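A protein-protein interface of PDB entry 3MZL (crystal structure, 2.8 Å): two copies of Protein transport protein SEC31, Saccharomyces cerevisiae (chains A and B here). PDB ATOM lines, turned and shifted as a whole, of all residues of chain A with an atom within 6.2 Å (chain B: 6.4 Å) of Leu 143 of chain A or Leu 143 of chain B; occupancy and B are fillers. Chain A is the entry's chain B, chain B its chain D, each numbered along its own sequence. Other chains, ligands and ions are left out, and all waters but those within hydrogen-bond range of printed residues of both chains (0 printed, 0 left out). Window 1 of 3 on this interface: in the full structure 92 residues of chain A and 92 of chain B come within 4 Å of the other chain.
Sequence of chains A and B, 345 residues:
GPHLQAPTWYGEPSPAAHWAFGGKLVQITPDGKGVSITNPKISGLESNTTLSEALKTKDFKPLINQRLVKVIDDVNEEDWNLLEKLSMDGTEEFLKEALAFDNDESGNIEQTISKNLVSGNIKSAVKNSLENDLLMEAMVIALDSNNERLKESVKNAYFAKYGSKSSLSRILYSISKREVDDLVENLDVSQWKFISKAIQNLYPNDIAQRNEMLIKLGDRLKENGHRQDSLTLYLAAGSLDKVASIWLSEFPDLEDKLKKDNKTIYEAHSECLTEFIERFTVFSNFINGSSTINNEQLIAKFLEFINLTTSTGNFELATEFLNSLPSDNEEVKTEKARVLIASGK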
ATOM      1  N   ALA A 138     -11.329   7.393 -14.195  1.00  0.00           N
ATOM      2  CA  ALA A 138     -12.169   6.541 -13.354  1.00  0.00           C
ATOM      3  C   ALA A 138     -13.534   7.184 -13.146  1.00  0.00           C
ATOM      4  O   ALA A 138     -14.534   6.490 -12.967  1.00  0.00           O
ATOM      5  CB  ALA A 138     -11.500   6.283 -12.019  1.00  0.00           C
ATOM      6  N   MET A 139     -13.560   8.516 -13.167  1.00  0.00           N
ATOM      7  CA  MET A 139     -14.785   9.284 -12.966  1.00  0.00           C
ATOM      8  C   MET A 139     -15.636   9.313 -14.219  1.00  0.00           C
ATOM      9  O   MET A 139     -16.846   9.099 -14.147  1.00  0.00           O
ATOM     10  CB  MET A 139     -14.465  10.711 -12.514  1.00  0.00           C
ATOM     11  CG  MET A 139     -14.078  10.819 -11.045  1.00  0.00           C
ATOM     12  SD  MET A 139     -13.693  12.504 -10.548  1.00  0.00           S
ATOM     13  CE  MET A 139     -13.291  12.258  -8.818  1.00  0.00           C
ATOM     14  N   VAL A 140     -14.998   9.572 -15.361  1.00  0.00           N
ATOM     15  CA  VAL A 140     -15.678   9.636 -16.661  1.00  0.00           C
ATOM     16  C   VAL A 140     -16.465   8.355 -16.926  1.00  0.00           C
ATOM     17  O   VAL A 140     -17.607   8.400 -17.393  1.00  0.00           O
ATOM     18  CB  VAL A 140     -14.680   9.896 -17.821  1.00  0.00           C
ATOM     19  CG1 VAL A 140     -15.398   9.931 -19.165  1.00  0.00           C
ATOM     20  CG2 VAL A 140     -13.932  11.202 -17.600  1.00  0.00           C
ATOM     21  N   ILE A 141     -15.843   7.219 -16.613  1.00  0.00           N
ATOM     22  CA  ILE A 141     -16.490   5.916 -16.713  1.00  0.00           C
ATOM     23  C   ILE A 141     -17.730   5.870 -15.822  1.00  0.00           C
ATOM     24  O   ILE A 141     -18.821   5.534 -16.291  1.00  0.00           O
ATOM     25  CB  ILE A 141     -15.527   4.772 -16.315  1.00  0.00           C
ATOM     26  CG1 ILE A 141     -14.317   4.728 -17.253  1.00  0.00           C
ATOM     27  CG2 ILE A 141     -16.255   3.433 -16.331  1.00  0.00           C
ATOM     28  CD1 ILE A 141     -13.229   3.751 -16.827  1.00  0.00           C
ATOM     29  N   ALA A 142     -17.551   6.234 -14.550  1.00  0.00           N
ATOM     30  CA  ALA A 142     -18.598   6.137 -13.525  1.00  0.00           C
ATOM     31  C   ALA A 142     -19.766   7.104 -13.728  1.00  0.00           C
ATOM     32  O   ALA A 142     -20.869   6.865 -13.239  1.00  0.00           O
ATOM     33  CB  ALA A 142     -17.989   6.328 -12.140  1.00  0.00           C
ATOM     34  N   LEU A 143     -19.514   8.188 -14.454  1.00  0.00           N
ATOM     35  CA  LEU A 143     -20.502   9.241 -14.672  1.00  0.00           C
ATOM     36  C   LEU A 143     -21.692   8.771 -15.524  1.00  0.00           C
ATOM     37  O   LEU A 143     -22.793   9.320 -15.419  1.00  0.00           O
ATOM     38  CB  LEU A 143     -19.821  10.451 -15.323  1.00  0.00           C
ATOM     39  CG  LEU A 143     -20.213  11.871 -14.910  1.00  0.00           C
ATOM     40  CD1 LEU A 143     -19.574  12.260 -13.589  1.00  0.00           C
ATOM     41  CD2 LEU A 143     -19.795  12.855 -15.981  1.00  0.00           C
ATOM     42  N   ASP A 144     -21.462   7.755 -16.355  1.00  0.00           N
ATOM     43  CA  ASP A 144     -22.484   7.232 -17.265  1.00  0.00           C
ATOM     44  C   ASP A 144     -23.023   5.867 -16.836  1.00  0.00           C
ATOM     45  O   ASP A 144     -23.886   5.297 -17.512  1.00  0.00           O
ATOM     46  CB  ASP A 144     -21.934   7.139 -18.695  1.00  0.00           C
ATOM     47  CG  ASP A 144     -21.813   8.499 -19.379  1.00  0.00           C
ATOM     48  OD1 ASP A 144     -22.448   9.477 -18.928  1.00  0.00           O
ATOM     49  OD2 ASP A 144     -21.080   8.583 -20.389  1.00  0.00           O
ATOM     50  N   SER A 145     -22.522   5.352 -15.715  1.00  0.00           N
ATOM     51  CA  SER A 145     -22.866   4.006 -15.250  1.00  0.00           C
ATOM     52  C   SER A 145     -24.330   3.853 -14.839  1.00  0.00           C
ATOM     53  O   SER A 145     -25.031   2.977 -15.357  1.00  0.00           O
ATOM     54  CB  SER A 145     -21.958   3.584 -14.090  1.00  0.00           C
ATOM     55  OG  SER A 145     -22.287   4.282 -12.899  1.00  0.00           O
ATOM     56  N   ASN A 146     -24.777   4.713 -13.919  1.00  0.00           N
ATOM     57  CA  ASN A 146     -26.074   4.573 -13.240  1.00  0.00           C
ATOM     58  C   ASN A 146     -26.217   3.186 -12.597  1.00  0.00           C
ATOM     59  O   ASN A 146     -27.293   2.581 -12.613  1.00  0.00           O
ATOM     60  CB  ASN A 146     -27.225   4.833 -14.212  1.00  0.00           C
ATOM     61  CG  ASN A 146     -27.347   6.293 -14.597  1.00  0.00           C
ATOM     62  OD1 ASN A 146     -26.891   7.178 -13.873  1.00  0.00           O
ATOM     63  ND2 ASN A 146     -27.963   6.555 -15.743  1.00  0.00           N
ATOM     64  N   GLU A 148     -24.313   2.508  -9.380  1.00  0.00           N
ATOM     65  CA  GLU A 148     -24.036   2.687  -7.945  1.00  0.00           C
ATOM     66  C   GLU A 148     -23.034   1.641  -7.437  1.00  0.00           C
ATOM     67  O   GLU A 148     -22.531   0.832  -8.224  1.00  0.00           O
ATOM     68  CB  GLU A 148     -25.334   2.687  -7.114  1.00  0.00           C
ATOM     69  CG  GLU A 148     -25.275   3.496  -5.813  1.00  0.00           C
ATOM     70  CD  GLU A 148     -25.177   4.999  -6.038  1.00  0.00           C
ATOM     71  OE1 GLU A 148     -24.558   5.682  -5.190  1.00  0.00           O
ATOM     72  OE2 GLU A 148     -25.714   5.501  -7.052  1.00  0.00           O
ATOM     73  N   LYS A 151     -19.844   3.879  -8.033  1.00  0.00           N
ATOM     74  CA  LYS A 151     -19.896   5.337  -7.879  1.00  0.00           C
ATOM     75  C   LYS A 151     -19.417   5.750  -6.487  1.00  0.00           C
ATOM     76  O   LYS A 151     -18.835   6.823  -6.311  1.00  0.00           O
ATOM     77  CB  LYS A 151     -21.316   5.865  -8.112  1.00  0.00           C
ATOM     78  CG  LYS A 151     -21.719   6.028  -9.572  1.00  0.00           C
ATOM     79  CD  LYS A 151     -23.025   6.813  -9.687  1.00  0.00           C
ATOM     80  CE  LYS A 151     -23.465   6.984 -11.136  1.00  0.00           C
ATOM     81  NZ  LYS A 151     -24.615   7.921 -11.266  1.00  0.00           N
ATOM     82  N   GLU A 152     -19.663   4.879  -5.512  1.00  0.00           N
ATOM     83  CA  GLU A 152     -19.271   5.108  -4.126  1.00  0.00           C
ATOM     84  C   GLU A 152     -17.813   4.714  -3.866  1.00  0.00           C
ATOM     85  O   GLU A 152     -17.240   5.081  -2.837  1.00  0.00           O
ATOM     86  CB  GLU A 152     -20.211   4.346  -3.185  1.00  0.00           C
ATOM     87  CG  GLU A 152     -20.607   5.116  -1.926  1.00  0.00           C
ATOM     88  CD  GLU A 152     -21.490   6.326  -2.216  1.00  0.00           C
ATOM     89  OE1 GLU A 152     -21.457   7.286  -1.418  1.00  0.00           O
ATOM     90  OE2 GLU A 152     -22.215   6.320  -3.236  1.00  0.00           O
ATOM     91  N   VAL A 154     -15.357   5.207  -6.395  1.00  0.00           N
ATOM     92  CA  VAL A 154     -14.635   6.295  -7.057  1.00  0.00           C
ATOM     93  C   VAL A 154     -14.519   7.494  -6.118  1.00  0.00           C
ATOM     94  O   VAL A 154     -13.455   8.111  -6.019  1.00  0.00           O
ATOM     95  CB  VAL A 154     -15.313   6.724  -8.387  1.00  0.00           C
ATOM     96  CG1 VAL A 154     -14.470   7.763  -9.113  1.00  0.00           C
ATOM     97  CG2 VAL A 154     -15.528   5.524  -9.291  1.00  0.00           C
ATOM     98  N   LYS A 155     -15.615   7.802  -5.424  1.00  0.00           N
ATOM     99  CA  LYS A 155     -15.646   8.902  -4.462  1.00  0.00           C
ATOM    100  C   LYS A 155     -14.682   8.677  -3.296  1.00  0.00           C
ATOM    101  O   LYS A 155     -13.883   9.559  -2.978  1.00  0.00           O
ATOM    102  CB  LYS A 155     -17.073   9.157  -3.967  1.00  0.00           C
ATOM    103  CG  LYS A 155     -17.955   9.851  -5.000  1.00  0.00           C
ATOM    104  CD  LYS A 155     -19.241  10.416  -4.406  1.00  0.00           C
ATOM    105  CE  LYS A 155     -20.337   9.365  -4.276  1.00  0.00           C
ATOM    106  NZ  LYS A 155     -21.623   9.964  -3.825  1.00  0.00           N
ATOM    107  N   ALA B 138     -15.961  19.223  -9.957  1.00  0.00           N
ATOM    108  CA  ALA B 138     -17.134  19.339 -10.830  1.00  0.00           C
ATOM    109  C   ALA B 138     -17.723  17.975 -11.162  1.00  0.00           C
ATOM    110  O   ALA B 138     -18.929  17.842 -11.363  1.00  0.00           O
ATOM    111  CB  ALA B 138     -16.780  20.075 -12.106  1.00  0.00           C
ATOM    112  N   MET B 139     -16.857  16.968 -11.220  1.00  0.00           N
ATOM    113  CA  MET B 139     -17.270  15.596 -11.468  1.00  0.00           C
ATOM    114  C   MET B 139     -17.890  14.969 -10.222  1.00  0.00           C
ATOM    115  O   MET B 139     -18.904  14.279 -10.318  1.00  0.00           O
ATOM    116  CB  MET B 139     -16.083  14.759 -11.952  1.00  0.00           C
ATOM    117  CG  MET B 139     -15.638  15.054 -13.378  1.00  0.00           C
ATOM    118  SD  MET B 139     -14.002  14.385 -13.743  1.00  0.00           S
ATOM    119  CE  MET B 139     -13.958  14.525 -15.529  1.00  0.00           C
ATOM    120  N   VAL B 140     -17.281  15.215  -9.061  1.00  0.00           N
ATOM    121  CA  VAL B 140     -17.781  14.689  -7.782  1.00  0.00           C
ATOM    122  C   VAL B 140     -19.158  15.269  -7.461  1.00  0.00           C
ATOM    123  O   VAL B 140     -19.999  14.592  -6.864  1.00  0.00           O
ATOM    124  CB  VAL B 140     -16.817  14.967  -6.592  1.00  0.00           C
ATOM    125  CG1 VAL B 140     -17.149  14.058  -5.413  1.00  0.00           C
ATOM    126  CG2 VAL B 140     -15.371  14.764  -6.995  1.00  0.00           C
ATOM    127  N   ILE B 141     -19.375  16.524  -7.860  1.00  0.00           N
ATOM    128  CA  ILE B 141     -20.686  17.162  -7.755  1.00  0.00           C
ATOM    129  C   ILE B 141     -21.715  16.397  -8.591  1.00  0.00           C
ATOM    130  O   ILE B 141     -22.707  15.904  -8.053  1.00  0.00           O
ATOM    131  CB  ILE B 141     -20.638  18.654  -8.182  1.00  0.00           C
ATOM    132  CG1 ILE B 141     -19.823  19.474  -7.178  1.00  0.00           C
ATOM    133  CG2 ILE B 141     -22.046  19.230  -8.295  1.00  0.00           C
ATOM    134  CD1 ILE B 141     -19.387  20.840  -7.690  1.00  0.00           C
ATOM    135  N   ALA B 142     -21.448  16.273  -9.894  1.00  0.00           N
ATOM    136  CA  ALA B 142     -22.391  15.681 -10.849  1.00  0.00           C
ATOM    137  C   ALA B 142     -22.625  14.176 -10.661  1.00  0.00           C
ATOM    138  O   ALA B 142     -23.611  13.625 -11.163  1.00  0.00           O
ATOM    139  CB  ALA B 142     -21.945  15.973 -12.272  1.00  0.00           C
ATOM    140  N   LEU B 143     -21.726  13.522  -9.931  1.00  0.00           N
ATOM    141  CA  LEU B 143     -21.776  12.071  -9.758  1.00  0.00           C
ATOM    142  C   LEU B 143     -23.005  11.622  -8.960  1.00  0.00           C
ATOM    143  O   LEU B 143     -23.345  10.439  -8.943  1.00  0.00           O
ATOM    144  CB  LEU B 143     -20.478  11.566  -9.114  1.00  0.00           C
ATOM    145  CG  LEU B 143     -20.010  10.130  -9.402  1.00  0.00           C
ATOM    146  CD1 LEU B 143     -19.654   9.916 -10.868  1.00  0.00           C
ATOM    147  CD2 LEU B 143     -18.826   9.766  -8.519  1.00  0.00           C
ATOM    148  N   ASP B 144     -23.665  12.579  -8.312  1.00  0.00           N
ATOM    149  CA  ASP B 144     -24.875  12.321  -7.530  1.00  0.00           C
ATOM    150  C   ASP B 144     -26.093  13.059  -8.093  1.00  0.00           C
ATOM    151  O   ASP B 144     -27.193  12.957  -7.546  1.00  0.00           O
ATOM    152  CB  ASP B 144     -24.661  12.724  -6.063  1.00  0.00           C
ATOM    153  CG  ASP B 144     -23.593  11.892  -5.368  1.00  0.00           C
ATOM    154  OD1 ASP B 144     -23.026  10.972  -5.995  1.00  0.00           O
ATOM    155  OD2 ASP B 144     -23.316  12.157  -4.178  1.00  0.00           O
ATOM    156  N   SER B 145     -25.894  13.793  -9.187  1.00  0.00           N
ATOM    157  CA  SER B 145     -26.944  14.641  -9.755  1.00  0.00           C
ATOM    158  C   SER B 145     -28.110  13.853 -10.356  1.00  0.00           C
ATOM    159  O   SER B 145     -29.271  14.121 -10.029  1.00  0.00           O
ATOM    160  CB  SER B 145     -26.363  15.611 -10.790  1.00  0.00           C
ATOM    161  OG  SER B 145     -25.814  14.916 -11.894  1.00  0.00           O
ATOM    162  N   ASN B 146     -27.791  12.889 -11.225  1.00  0.00           N
ATOM    163  CA  ASN B 146     -28.788  12.061 -11.929  1.00  0.00           C
ATOM    164  C   ASN B 146     -29.877  12.882 -12.641  1.00  0.00           C
ATOM    165  O   ASN B 146     -31.038  12.466 -12.719  1.00  0.00           O
ATOM    166  CB  ASN B 146     -29.436  11.076 -10.955  1.00  0.00           C
ATOM    167  CG  ASN B 146     -28.484   9.983 -10.511  1.00  0.00           C
ATOM    168  OD1 ASN B 146     -27.508   9.679 -11.196  1.00  0.00           O
ATOM    169  ND2 ASN B 146     -28.765   9.385  -9.359  1.00  0.00           N
ATOM    170  N   LEU B 150     -26.433  18.240 -17.380  1.00  0.00           N
ATOM    171  CA  LEU B 150     -25.268  18.697 -16.626  1.00  0.00           C
ATOM    172  C   LEU B 150     -24.102  17.730 -16.763  1.00  0.00           C
ATOM    173  O   LEU B 150     -22.982  18.147 -17.055  1.00  0.00           O
ATOM    174  CB  LEU B 150     -25.612  18.892 -15.147  1.00  0.00           C
ATOM    175  CG  LEU B 150     -26.337  20.179 -14.747  1.00  0.00           C
ATOM    176  CD1 LEU B 150     -27.847  19.958 -14.683  1.00  0.00           C
ATOM    177  CD2 LEU B 150     -25.813  20.667 -13.409  1.00  0.00           C
ATOM    178  N   LYS B 151     -24.378  16.442 -16.555  1.00  0.00           N
ATOM    179  CA  LYS B 151     -23.373  15.383 -16.658  1.00  0.00           C
ATOM    180  C   LYS B 151     -22.601  15.437 -17.976  1.00  0.00           C
ATOM    181  O   LYS B 151     -21.415  15.104 -18.026  1.00  0.00           O
ATOM    182  CB  LYS B 151     -24.025  14.008 -16.502  1.00  0.00           C
ATOM    183  CG  LYS B 151     -24.396  13.641 -15.075  1.00  0.00           C
ATOM    184  CD  LYS B 151     -24.898  12.204 -15.008  1.00  0.00           C
ATOM    185  CE  LYS B 151     -25.034  11.723 -13.574  1.00  0.00           C
ATOM    186  NZ  LYS B 151     -25.526  10.320 -13.514  1.00  0.00           N
ATOM    187  N   GLU B 152     -23.284  15.866 -19.033  1.00  0.00           N
ATOM    188  CA  GLU B 152     -22.680  15.986 -20.352  1.00  0.00           C
ATOM    189  C   GLU B 152     -21.659  17.123 -20.403  1.00  0.00           C
ATOM    190  O   GLU B 152     -20.566  16.951 -20.941  1.00  0.00           O
ATOM    191  CB  GLU B 152     -23.764  16.173 -21.421  1.00  0.00           C
ATOM    192  CG  GLU B 152     -23.482  15.447 -22.740  1.00  0.00           C
ATOM    193  CD  GLU B 152     -23.557  13.924 -22.624  1.00  0.00           C
ATOM    194  OE1 GLU B 152     -23.071  13.238 -23.550  1.00  0.00           O
ATOM    195  OE2 GLU B 152     -24.097  13.409 -21.620  1.00  0.00           O
ATOM    196  N   VAL B 154     -19.932  18.335 -18.007  1.00  0.00           N
ATOM    197  CA  VAL B 154     -18.765  17.930 -17.231  1.00  0.00           C
ATOM    198  C   VAL B 154     -17.849  17.067 -18.100  1.00  0.00           C
ATOM    199  O   VAL B 154     -16.626  17.196 -18.040  1.00  0.00           O
ATOM    200  CB  VAL B 154     -19.153  17.150 -15.951  1.00  0.00           C
ATOM    201  CG1 VAL B 154     -18.026  17.204 -14.939  1.00  0.00           C
ATOM    202  CG2 VAL B 154     -20.410  17.721 -15.330  1.00  0.00           C
ATOM    203  N   LYS B 155     -18.453  16.197 -18.908  1.00  0.00           N
ATOM    204  CA  LYS B 155     -17.716  15.378 -19.868  1.00  0.00           C
ATOM    205  C   LYS B 155     -17.129  16.231 -20.989  1.00  0.00           C
ATOM    206  O   LYS B 155     -15.975  16.045 -21.367  1.00  0.00           O
ATOM    207  CB  LYS B 155     -18.609  14.276 -20.447  1.00  0.00           C
ATOM    208  CG  LYS B 155     -18.913  13.140 -19.473  1.00  0.00           C
ATOM    209  CD  LYS B 155     -19.755  12.040 -20.110  1.00  0.00           C
ATOM    210  CE  LYS B 155     -21.217  12.442 -20.237  1.00  0.00           C
ATOM    211  NZ  LYS B 155     -22.030  11.399 -20.918  1.00  0.00           N
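O of Leu 143 of chain A sits at hydrogen-bond distance from NZ of Lys 151 of chain B, at 3.5 Å. NZ of Lys 151 of chain A lies close to NZ of Lys 151 of chain B, 3.4 Å away. NZ of Lys 151 of chain A sits at hydrogen-bond distance from OD1 of Asn 146 of chain B, 3.4 Å away. The side-chain carboxylate (OD1) of Asp 144 of chain B lies within salt-bridge range of the side-chain amino group (NZ) of Lys 155 of chain A, 2.8 Å away. NZ of Lys 155 of chain B lies within salt-bridge range of OD1 of Asp 144 of chain A, at 2.8 Å. OD1 of Asn 146 of chain A lies within hydrogen-bond range of NZ of Lys 151 of chain B, 3.4 Å away. SD of Met 139 of chain B sits close to SD of Met 139 of chain A, 3.7 Å away.
OE1 of Glu 152 of chain A is in salt-bridge range of NZ of Lys 155 of chain A, at 3.6 Å. NZ of Lys 151 of chain B lies within hydrogen-bond range of OD1 of Asn 146 of chain B (3.1 Å). The side-chain carboxylate (OE2) of Glu 152 of chain B lies within salt-bridge range of the side-chain amino group (NZ) of Lys 155 of chain B (3.0 Å).
Hydrophobic or aromatic side chains of chain B within 4 Å of the printed part of chain A: Met 139, Val 140 and Leu 143. Of the 14 printed residues of chain A, 7 touch a printed residue of chain B. Hydrophobic or aromatic side chains of chain A within 4 Å of the printed part of chain B: Met 139, Val 140 and Leu 143. Among the printed residues, 15 pairs touch across the chains. Among the printed residues, Asp or Glu carboxylates within 4 Å of a Lys or Arg side-chain nitrogen of the other chain: Asp 144 of chain A with Lys 155 of chain B and Lys 155 of chain A with Asp 144 of chain B.
Val 140 of chain B touches Met 139 of chain A. Val 140 of chain A touches Met 139 of chain B. CD1 of Leu 143 of chain A touches O of Met 139 of chain B, 3.9 Å away. Leu 143 of chain B touches Leu 143 of chain A (CD1 to CD1, 3.6 Å). Leu 143 of chain A touches Lys 155 of chain B (CD2 to CG, 3.6 Å). Asn 146 of chain B touches Asn 146 of chain A. Lys 151 of chain A touches Leu 143 of chain B. CD2 of Leu 143 of chain B touches CG of Lys 155 of chain A (3.6 Å).
Leu 143 of chain A touches just these residues of chain B: Met 139 (3.9 Å), Leu 143 (3.6 Å), Lys 151 (3.4 Å) and Lys 155 (3.6 Å). Of the printed residues of chain A, Leu 143 of chain B touches Leu 143 (3.6 Å), Lys 151 (3.7 Å) and Lys 155 (3.6 Å). Printed residues of chain A within 4 Å of Val 140 of chain B: Met 139. Of the printed residues of chain B, Asn 146 of chain A touches Asn 146 (3.7 Å) and Lys 151 (3.4 Å). Printed residues of chain B within 4 Å of Val 140 of chain A: Met 139 (3.9 Å). The nearest residue of chain B that does not touch Leu 143 of chain A is Val 154 of chain B (4.3 Å). The nearest printed residue of chain B that does not touch Asn 146 of chain A is Leu 143 of chain B (6.9 Å).
Met 139 of chain A touches Val 140 of chain B, and with the chains exchanged Val 140 of chain A touches Met 139 of chain B. Leu 143 of chain A touches Lys 151 of chain B, and with the chains exchanged Lys 151 of chain A touches Leu 143 of chain B. Asn 146 of chain A touches Lys 151 of chain B, and with the chains exchanged Lys 151 of chain A touches Asn 146 of chain B. Lys 151 of chain B touches its own counterpart, Lys 151 of chain A. Positions printed for both chains: 138, 139, 140, 141, 142, 143, 144, 145, 146, 151, 152, 154 and 155. Of the 15 pairs that touch across the chains among the printed residues, 14 have their exchanged pair printed and touching as well.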
